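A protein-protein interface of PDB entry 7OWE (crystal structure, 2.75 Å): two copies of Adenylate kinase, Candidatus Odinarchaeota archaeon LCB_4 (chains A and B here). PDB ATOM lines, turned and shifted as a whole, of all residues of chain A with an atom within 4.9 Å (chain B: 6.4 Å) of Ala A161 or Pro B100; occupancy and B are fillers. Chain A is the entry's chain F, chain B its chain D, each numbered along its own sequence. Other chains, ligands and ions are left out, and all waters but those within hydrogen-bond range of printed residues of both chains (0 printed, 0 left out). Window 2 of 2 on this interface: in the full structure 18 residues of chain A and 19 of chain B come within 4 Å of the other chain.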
ATOM      1  N   VAL A 157      20.780  10.817  27.015  1.00  0.00           N
ATOM      2  CA  VAL A 157      20.587  12.246  26.787  1.00  0.00           C
ATOM      3  C   VAL A 157      21.567  12.763  25.742  1.00  0.00           C
ATOM      4  O   VAL A 157      21.211  13.588  24.892  1.00  0.00           O
ATOM      5  CB  VAL A 157      20.717  13.021  28.110  1.00  0.00           C
ATOM      6  CG1 VAL A 157      20.832  14.514  27.841  1.00  0.00           C
ATOM      7  CG2 VAL A 157      19.527  12.722  28.999  1.00  0.00           C
ATOM      8  N   SER A 158      22.812  12.317  25.778  1.00  0.00           N
ATOM      9  CA  SER A 158      23.770  12.827  24.808  1.00  0.00           C
ATOM     10  C   SER A 158      23.389  12.488  23.385  1.00  0.00           C
ATOM     11  O   SER A 158      23.432  13.330  22.483  1.00  0.00           O
ATOM     12  CB  SER A 158      25.149  12.259  25.095  1.00  0.00           C
ATOM     13  OG  SER A 158      25.575  12.629  26.387  1.00  0.00           O
ATOM     14  N   TYR A 159      22.998  11.243  23.185  1.00  0.00           N
ATOM     15  CA  TYR A 159      22.608  10.803  21.866  1.00  0.00           C
ATOM     16  C   TYR A 159      21.369  11.525  21.393  1.00  0.00           C
ATOM     17  O   TYR A 159      21.256  11.885  20.231  1.00  0.00           O
ATOM     18  CB  TYR A 159      22.450   9.294  21.829  1.00  0.00           C
ATOM     19  CG  TYR A 159      23.782   8.599  21.857  1.00  0.00           C
ATOM     20  CD1 TYR A 159      24.744   8.880  20.905  1.00  0.00           C
ATOM     21  CD2 TYR A 159      24.083   7.673  22.832  1.00  0.00           C
ATOM     22  CE1 TYR A 159      25.968   8.254  20.924  1.00  0.00           C
ATOM     23  CE2 TYR A 159      25.307   7.041  22.858  1.00  0.00           C
ATOM     24  CZ  TYR A 159      26.244   7.336  21.900  1.00  0.00           C
ATOM     25  OH  TYR A 159      27.464   6.713  21.913  1.00  0.00           O
ATOM     26  N   SER A 160      20.433  11.736  22.304  1.00  0.00           N
ATOM     27  CA  SER A 160      19.214  12.422  21.952  1.00  0.00           C
ATOM     28  C   SER A 160      19.519  13.833  21.509  1.00  0.00           C
ATOM     29  O   SER A 160      18.976  14.308  20.525  1.00  0.00           O
ATOM     30  CB  SER A 160      18.274  12.474  23.144  1.00  0.00           C
ATOM     31  OG  SER A 160      17.176  13.315  22.870  1.00  0.00           O
ATOM     32  N   ALA A 161      20.404  14.503  22.226  1.00  0.00           N
ATOM     33  CA  ALA A 161      20.737  15.863  21.866  1.00  0.00           C
ATOM     34  C   ALA A 161      21.352  15.865  20.494  1.00  0.00           C
ATOM     35  O   ALA A 161      21.047  16.703  19.663  1.00  0.00           O
ATOM     36  CB  ALA A 161      21.711  16.437  22.866  1.00  0.00           C
ATOM     37  N   ILE A 162      22.237  14.911  20.266  1.00  0.00           N
ATOM     38  CA  ILE A 162      22.896  14.785  18.977  1.00  0.00           C
ATOM     39  C   ILE A 162      22.022  14.367  17.804  1.00  0.00           C
ATOM     40  O   ILE A 162      22.244  14.788  16.680  1.00  0.00           O
ATOM     41  CB  ILE A 162      24.079  13.808  19.048  1.00  0.00           C
ATOM     42  CG1 ILE A 162      25.053  14.240  20.133  1.00  0.00           C
ATOM     43  CG2 ILE A 162      24.801  13.743  17.716  1.00  0.00           C
ATOM     44  CD1 ILE A 162      26.348  13.467  20.106  1.00  0.00           C
ATOM     45  N   ASN A 163      21.062  13.496  18.064  1.00  0.00           N
ATOM     46  CA  ASN A 163      20.248  12.896  17.010  1.00  0.00           C
ATOM     47  C   ASN A 163      18.761  13.217  17.108  1.00  0.00           C
ATOM     48  O   ASN A 163      17.959  12.581  16.412  1.00  0.00           O
ATOM     49  CB  ASN A 163      20.431  11.373  17.001  1.00  0.00           C
ATOM     50  CG  ASN A 163      21.809  10.953  16.540  1.00  0.00           C
ATOM     51  OD1 ASN A 163      22.580  10.380  17.307  1.00  0.00           O
ATOM     52  ND2 ASN A 163      22.125  11.233  15.279  1.00  0.00           N
ATOM     53  N   GLN A 164      18.361  14.174  17.942  1.00  0.00           N
ATOM     54  CA  GLN A 164      16.982  14.664  17.933  1.00  0.00           C
ATOM     55  C   GLN A 164      15.981  13.526  18.145  1.00  0.00           C
ATOM     56  O   GLN A 164      14.925  13.478  17.512  1.00  0.00           O
ATOM     57  CB  GLN A 164      16.703  15.411  16.621  1.00  0.00           C
ATOM     58  CG  GLN A 164      15.358  16.117  16.529  1.00  0.00           C
ATOM     59  CD  GLN A 164      14.441  15.512  15.472  1.00  0.00           C
ATOM     60  OE1 GLN A 164      14.882  14.782  14.584  1.00  0.00           O
ATOM     61  NE2 GLN A 164      13.153  15.816  15.569  1.00  0.00           N
ATOM     62  N   PRO B  96      14.736  17.023  22.786  1.00  0.00           N
ATOM     63  CA  PRO B  96      15.679  18.133  22.979  1.00  0.00           C
ATOM     64  C   PRO B  96      15.089  19.455  22.513  1.00  0.00           C
ATOM     65  O   PRO B  96      14.537  19.555  21.416  1.00  0.00           O
ATOM     66  CB  PRO B  96      16.893  17.734  22.127  1.00  0.00           C
ATOM     67  CG  PRO B  96      16.697  16.302  21.776  1.00  0.00           C
ATOM     68  CD  PRO B  96      15.221  16.061  21.782  1.00  0.00           C
ATOM     69  N   LEU B  98      17.003  21.944  21.861  1.00  0.00           N
ATOM     70  CA  LEU B  98      17.992  22.438  20.917  1.00  0.00           C
ATOM     71  C   LEU B  98      18.600  21.266  20.159  1.00  0.00           C
ATOM     72  O   LEU B  98      18.900  20.222  20.746  1.00  0.00           O
ATOM     73  CB  LEU B  98      19.086  23.233  21.634  1.00  0.00           C
ATOM     74  CG  LEU B  98      18.566  24.443  22.413  1.00  0.00           C
ATOM     75  CD1 LEU B  98      19.695  25.160  23.131  1.00  0.00           C
ATOM     76  CD2 LEU B  98      17.833  25.402  21.485  1.00  0.00           C
ATOM     77  N   ILE B  99      18.765  21.446  18.851  1.00  0.00           N
ATOM     78  CA  ILE B  99      19.311  20.423  17.959  1.00  0.00           C
ATOM     79  C   ILE B  99      20.365  21.091  17.084  1.00  0.00           C
ATOM     80  O   ILE B  99      20.197  22.261  16.711  1.00  0.00           O
ATOM     81  CB  ILE B  99      18.205  19.778  17.114  1.00  0.00           C
ATOM     82  CG1 ILE B  99      17.489  20.852  16.295  1.00  0.00           C
ATOM     83  CG2 ILE B  99      17.231  19.029  18.011  1.00  0.00           C
ATOM     84  CD1 ILE B  99      16.430  20.311  15.369  1.00  0.00           C
ATOM     85  N   PRO B 100      21.446  20.388  16.713  1.00  0.00           N
ATOM     86  CA  PRO B 100      22.632  21.064  16.156  1.00  0.00           C
ATOM     87  C   PRO B 100      22.335  22.218  15.210  1.00  0.00           C
ATOM     88  O   PRO B 100      22.978  23.273  15.302  1.00  0.00           O
ATOM     89  CB  PRO B 100      23.364  19.924  15.431  1.00  0.00           C
ATOM     90  CG  PRO B 100      22.999  18.703  16.218  1.00  0.00           C
ATOM     91  CD  PRO B 100      21.576  18.918  16.688  1.00  0.00           C
ATOM     92  N   GLU B 101      21.366  22.043  14.307  1.00  0.00           N
ATOM     93  CA  GLU B 101      20.998  23.135  13.413  1.00  0.00           C
ATOM     94  C   GLU B 101      20.696  24.397  14.210  1.00  0.00           C
ATOM     95  O   GLU B 101      21.290  25.458  13.978  1.00  0.00           O
ATOM     96  CB  GLU B 101      19.781  22.754  12.564  1.00  0.00           C
ATOM     97  CG  GLU B 101      19.973  21.584  11.614  1.00  0.00           C
ATOM     98  CD  GLU B 101      19.772  20.240  12.289  1.00  0.00           C
ATOM     99  OE1 GLU B 101      19.780  20.196  13.536  1.00  0.00           O
ATOM    100  OE2 GLU B 101      19.603  19.229  11.575  1.00  0.00           O
ATOM    101  N   THR B 102      19.778  24.293  15.171  1.00  0.00           N
ATOM    102  CA  THR B 102      19.327  25.472  15.896  1.00  0.00           C
ATOM    103  C   THR B 102      20.445  26.075  16.737  1.00  0.00           C
ATOM    104  O   THR B 102      20.563  27.302  16.821  1.00  0.00           O
ATOM    105  CB  THR B 102      18.117  25.118  16.762  1.00  0.00           C
ATOM    106  OG1 THR B 102      18.419  23.982  17.578  1.00  0.00           O
ATOM    107  CG2 THR B 102      16.911  24.804  15.879  1.00  0.00           C
ATOM    108  N   ILE B 103      21.285  25.246  17.366  1.00  0.00           N
ATOM    109  CA  ILE B 103      22.368  25.815  18.162  1.00  0.00           C
ATOM    110  C   ILE B 103      23.323  26.591  17.264  1.00  0.00           C
ATOM    111  O   ILE B 103      23.762  27.694  17.608  1.00  0.00           O
ATOM    112  CB  ILE B 103      23.123  24.736  18.956  1.00  0.00           C
ATOM    113  CG1 ILE B 103      22.244  24.094  20.022  1.00  0.00           C
ATOM    114  CG2 ILE B 103      24.323  25.366  19.653  1.00  0.00           C
ATOM    115  CD1 ILE B 103      22.839  22.882  20.634  1.00  0.00           C
ATOM    116  N   ASN B 104      23.665  26.029  16.101  1.00  0.00           N
ATOM    117  CA  ASN B 104      24.573  26.732  15.204  1.00  0.00           C
ATOM    118  C   ASN B 104      23.924  27.972  14.598  1.00  0.00           C
ATOM    119  O   ASN B 104      24.640  28.891  14.188  1.00  0.00           O
ATOM    120  CB  ASN B 104      25.069  25.794  14.103  1.00  0.00           C
ATOM    121  CG  ASN B 104      26.220  26.385  13.307  1.00  0.00           C
ATOM    122  OD1 ASN B 104      26.859  27.347  13.736  1.00  0.00           O
ATOM    123  ND2 ASN B 104      26.489  25.811  12.140  1.00  0.00           N
ATOM    124  N   ILE B 105      22.591  28.027  14.541  1.00  0.00           N
ATOM    125  CA  ILE B 105      21.928  29.246  14.083  1.00  0.00           C
ATOM    126  C   ILE B 105      21.986  30.323  15.163  1.00  0.00           C
ATOM    127  O   ILE B 105      22.352  31.473  14.894  1.00  0.00           O
ATOM    128  CB  ILE B 105      20.473  28.958  13.667  1.00  0.00           C
ATOM    129  CG1 ILE B 105      20.423  28.006  12.473  1.00  0.00           C
ATOM    130  CG2 ILE B 105      19.760  30.262  13.313  1.00  0.00           C
ATOM    131  CD1 ILE B 105      19.022  27.506  12.146  1.00  0.00           C
ATOM    132  N   PHE B 155      20.942  17.711  29.310  1.00  0.00           N
ATOM    133  CA  PHE B 155      20.873  18.268  27.961  1.00  0.00           C
ATOM    134  C   PHE B 155      21.776  19.492  27.849  1.00  0.00           C
ATOM    135  O   PHE B 155      22.511  19.648  26.860  1.00  0.00           O
ATOM    136  CB  PHE B 155      19.425  18.597  27.599  1.00  0.00           C
ATOM    137  CG  PHE B 155      18.681  17.452  26.976  1.00  0.00           C
ATOM    138  CD1 PHE B 155      18.950  17.061  25.675  1.00  0.00           C
ATOM    139  CD2 PHE B 155      17.710  16.768  27.688  1.00  0.00           C
ATOM    140  CE1 PHE B 155      18.269  16.009  25.095  1.00  0.00           C
ATOM    141  CE2 PHE B 155      17.025  15.715  27.112  1.00  0.00           C
ATOM    142  CZ  PHE B 155      17.306  15.335  25.812  1.00  0.00           C
ATOM    143  N   SER B 158      25.368  18.547  27.505  1.00  0.00           N
ATOM    144  CA  SER B 158      25.652  18.015  26.173  1.00  0.00           C
ATOM    145  C   SER B 158      25.819  19.144  25.159  1.00  0.00           C
ATOM    146  O   SER B 158      26.807  19.192  24.406  1.00  0.00           O
ATOM    147  CB  SER B 158      24.540  17.061  25.739  1.00  0.00           C
ATOM    148  OG  SER B 158      24.553  15.876  26.515  1.00  0.00           O
ATOM    149  N   TYR B 159      24.847  20.059  25.115  1.00  0.00           N
ATOM    150  CA  TYR B 159      24.954  21.201  24.214  1.00  0.00           C
ATOM    151  C   TYR B 159      26.280  21.929  24.410  1.00  0.00           C
ATOM    152  O   TYR B 159      26.956  22.289  23.436  1.00  0.00           O
ATOM    153  CB  TYR B 159      23.785  22.160  24.440  1.00  0.00           C
ATOM    154  CG  TYR B 159      22.409  21.557  24.237  1.00  0.00           C
ATOM    155  CD1 TYR B 159      22.206  20.473  23.389  1.00  0.00           C
ATOM    156  CD2 TYR B 159      21.312  22.084  24.895  1.00  0.00           C
ATOM    157  CE1 TYR B 159      20.935  19.934  23.212  1.00  0.00           C
ATOM    158  CE2 TYR B 159      20.048  21.556  24.725  1.00  0.00           C
ATOM    159  CZ  TYR B 159      19.860  20.484  23.888  1.00  0.00           C
ATOM    160  OH  TYR B 159      18.590  19.973  23.730  1.00  0.00           O
ATOM    161  N   ILE B 162      29.248  20.288  22.992  1.00  0.00           N
ATOM    162  CA  ILE B 162      29.310  20.348  21.537  1.00  0.00           C
ATOM    163  C   ILE B 162      29.694  21.740  21.025  1.00  0.00           C
ATOM    164  O   ILE B 162      30.384  21.846  20.003  1.00  0.00           O
ATOM    165  CB  ILE B 162      27.972  19.877  20.936  1.00  0.00           C
ATOM    166  CG1 ILE B 162      27.826  18.364  21.129  1.00  0.00           C
ATOM    167  CG2 ILE B 162      27.886  20.245  19.463  1.00  0.00           C
ATOM    168  CD1 ILE B 162      26.461  17.816  20.776  1.00  0.00           C
ATOM    169  N   ASN B 163      29.293  22.825  21.713  1.00  0.00           N
ATOM    170  CA  ASN B 163      29.299  24.139  21.075  1.00  0.00           C
ATOM    171  C   ASN B 163      30.071  25.229  21.818  1.00  0.00           C
ATOM    172  O   ASN B 163      29.878  26.416  21.524  1.00  0.00           O
ATOM    173  CB  ASN B 163      27.852  24.610  20.862  1.00  0.00           C
ATOM    174  CG  ASN B 163      27.136  23.818  19.797  1.00  0.00           C
ATOM    175  OD1 ASN B 163      26.353  22.918  20.095  1.00  0.00           O
ATOM    176  ND2 ASN B 163      27.402  24.149  18.540  1.00  0.00           N
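Ser A158 touches its own counterpart, Ser B158.
Ile B162 touches its own counterpart, Ile A162.
4 positions are printed for both chains.
Of the 9 pairs that touch across the chains among the printed residues, 2 have their exchanged pair printed and touching as well.
Printed residues of chain B within 4 Å of Ala A161: Pro B100 (3.7 Å), Phe B155 (3.9 Å) and Tyr B159 (3.6 Å).
Of the printed residues of chain A, Pro B100 touches Ala A161.
Printed residues of chain A within 4 Å of Ser B158: Ser A158.
Of the printed residues of chain A, Ile B162 touches Ile A162 (3.9 Å).
Printed residues of chain B within 4 Å of Ser A158: Ser B158 (3.4 Å).
Ile B105 touches none of the printed residues of chain A.
Leu B98 touches none of the printed residues of chain A.
Among the printed residues, pairs that only touch across the chains: Ser A160 with Pro B96, Val A157 with Phe B155, Ser A160 with Phe B155, Ala A161 with Tyr B159, Ala A161 with Pro B100, Gln A164 with Ile B99, Ala A161 with Phe B155 and Ile A162 with Ile B162.
Hydrophobic or aromatic side chains of chain A that line the printed part of chain B: Val A157, Ala A161 and Ile A162.
Hydrophobic or aromatic side chains of chain B that line the printed part of chain A: Pro B96, Ile B99, Pro B100, Phe B155, Tyr B159 and Ile B162.
Among the printed residues, 9 pairs touch across the chains.
Among the printed residues, no Asp or Glu carboxylate lies within 4 Å of a Lys or Arg side-chain nitrogen of the other chain.
The side-chain hydroxyl (OH) of Tyr B159 is in hydrogen-bond range of the backbone carbonyl oxygen (O) of Leu B98, 3.0 Å away.
The side-chain hydroxyl (OG1) of Thr B102 lies within hydrogen-bond range of the backbone carbonyl oxygen (O) of Ile B99 (2.6 Å).
The backbone carbonyl oxygen (O) of Tyr B159 sits close to the side-chain amide oxygen (OD1) of Asn B163.
The side-chain hydroxyl (OG) of Ser A158 lies within hydrogen-bond range of the side-chain hydroxyl (OG) of Ser B158.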
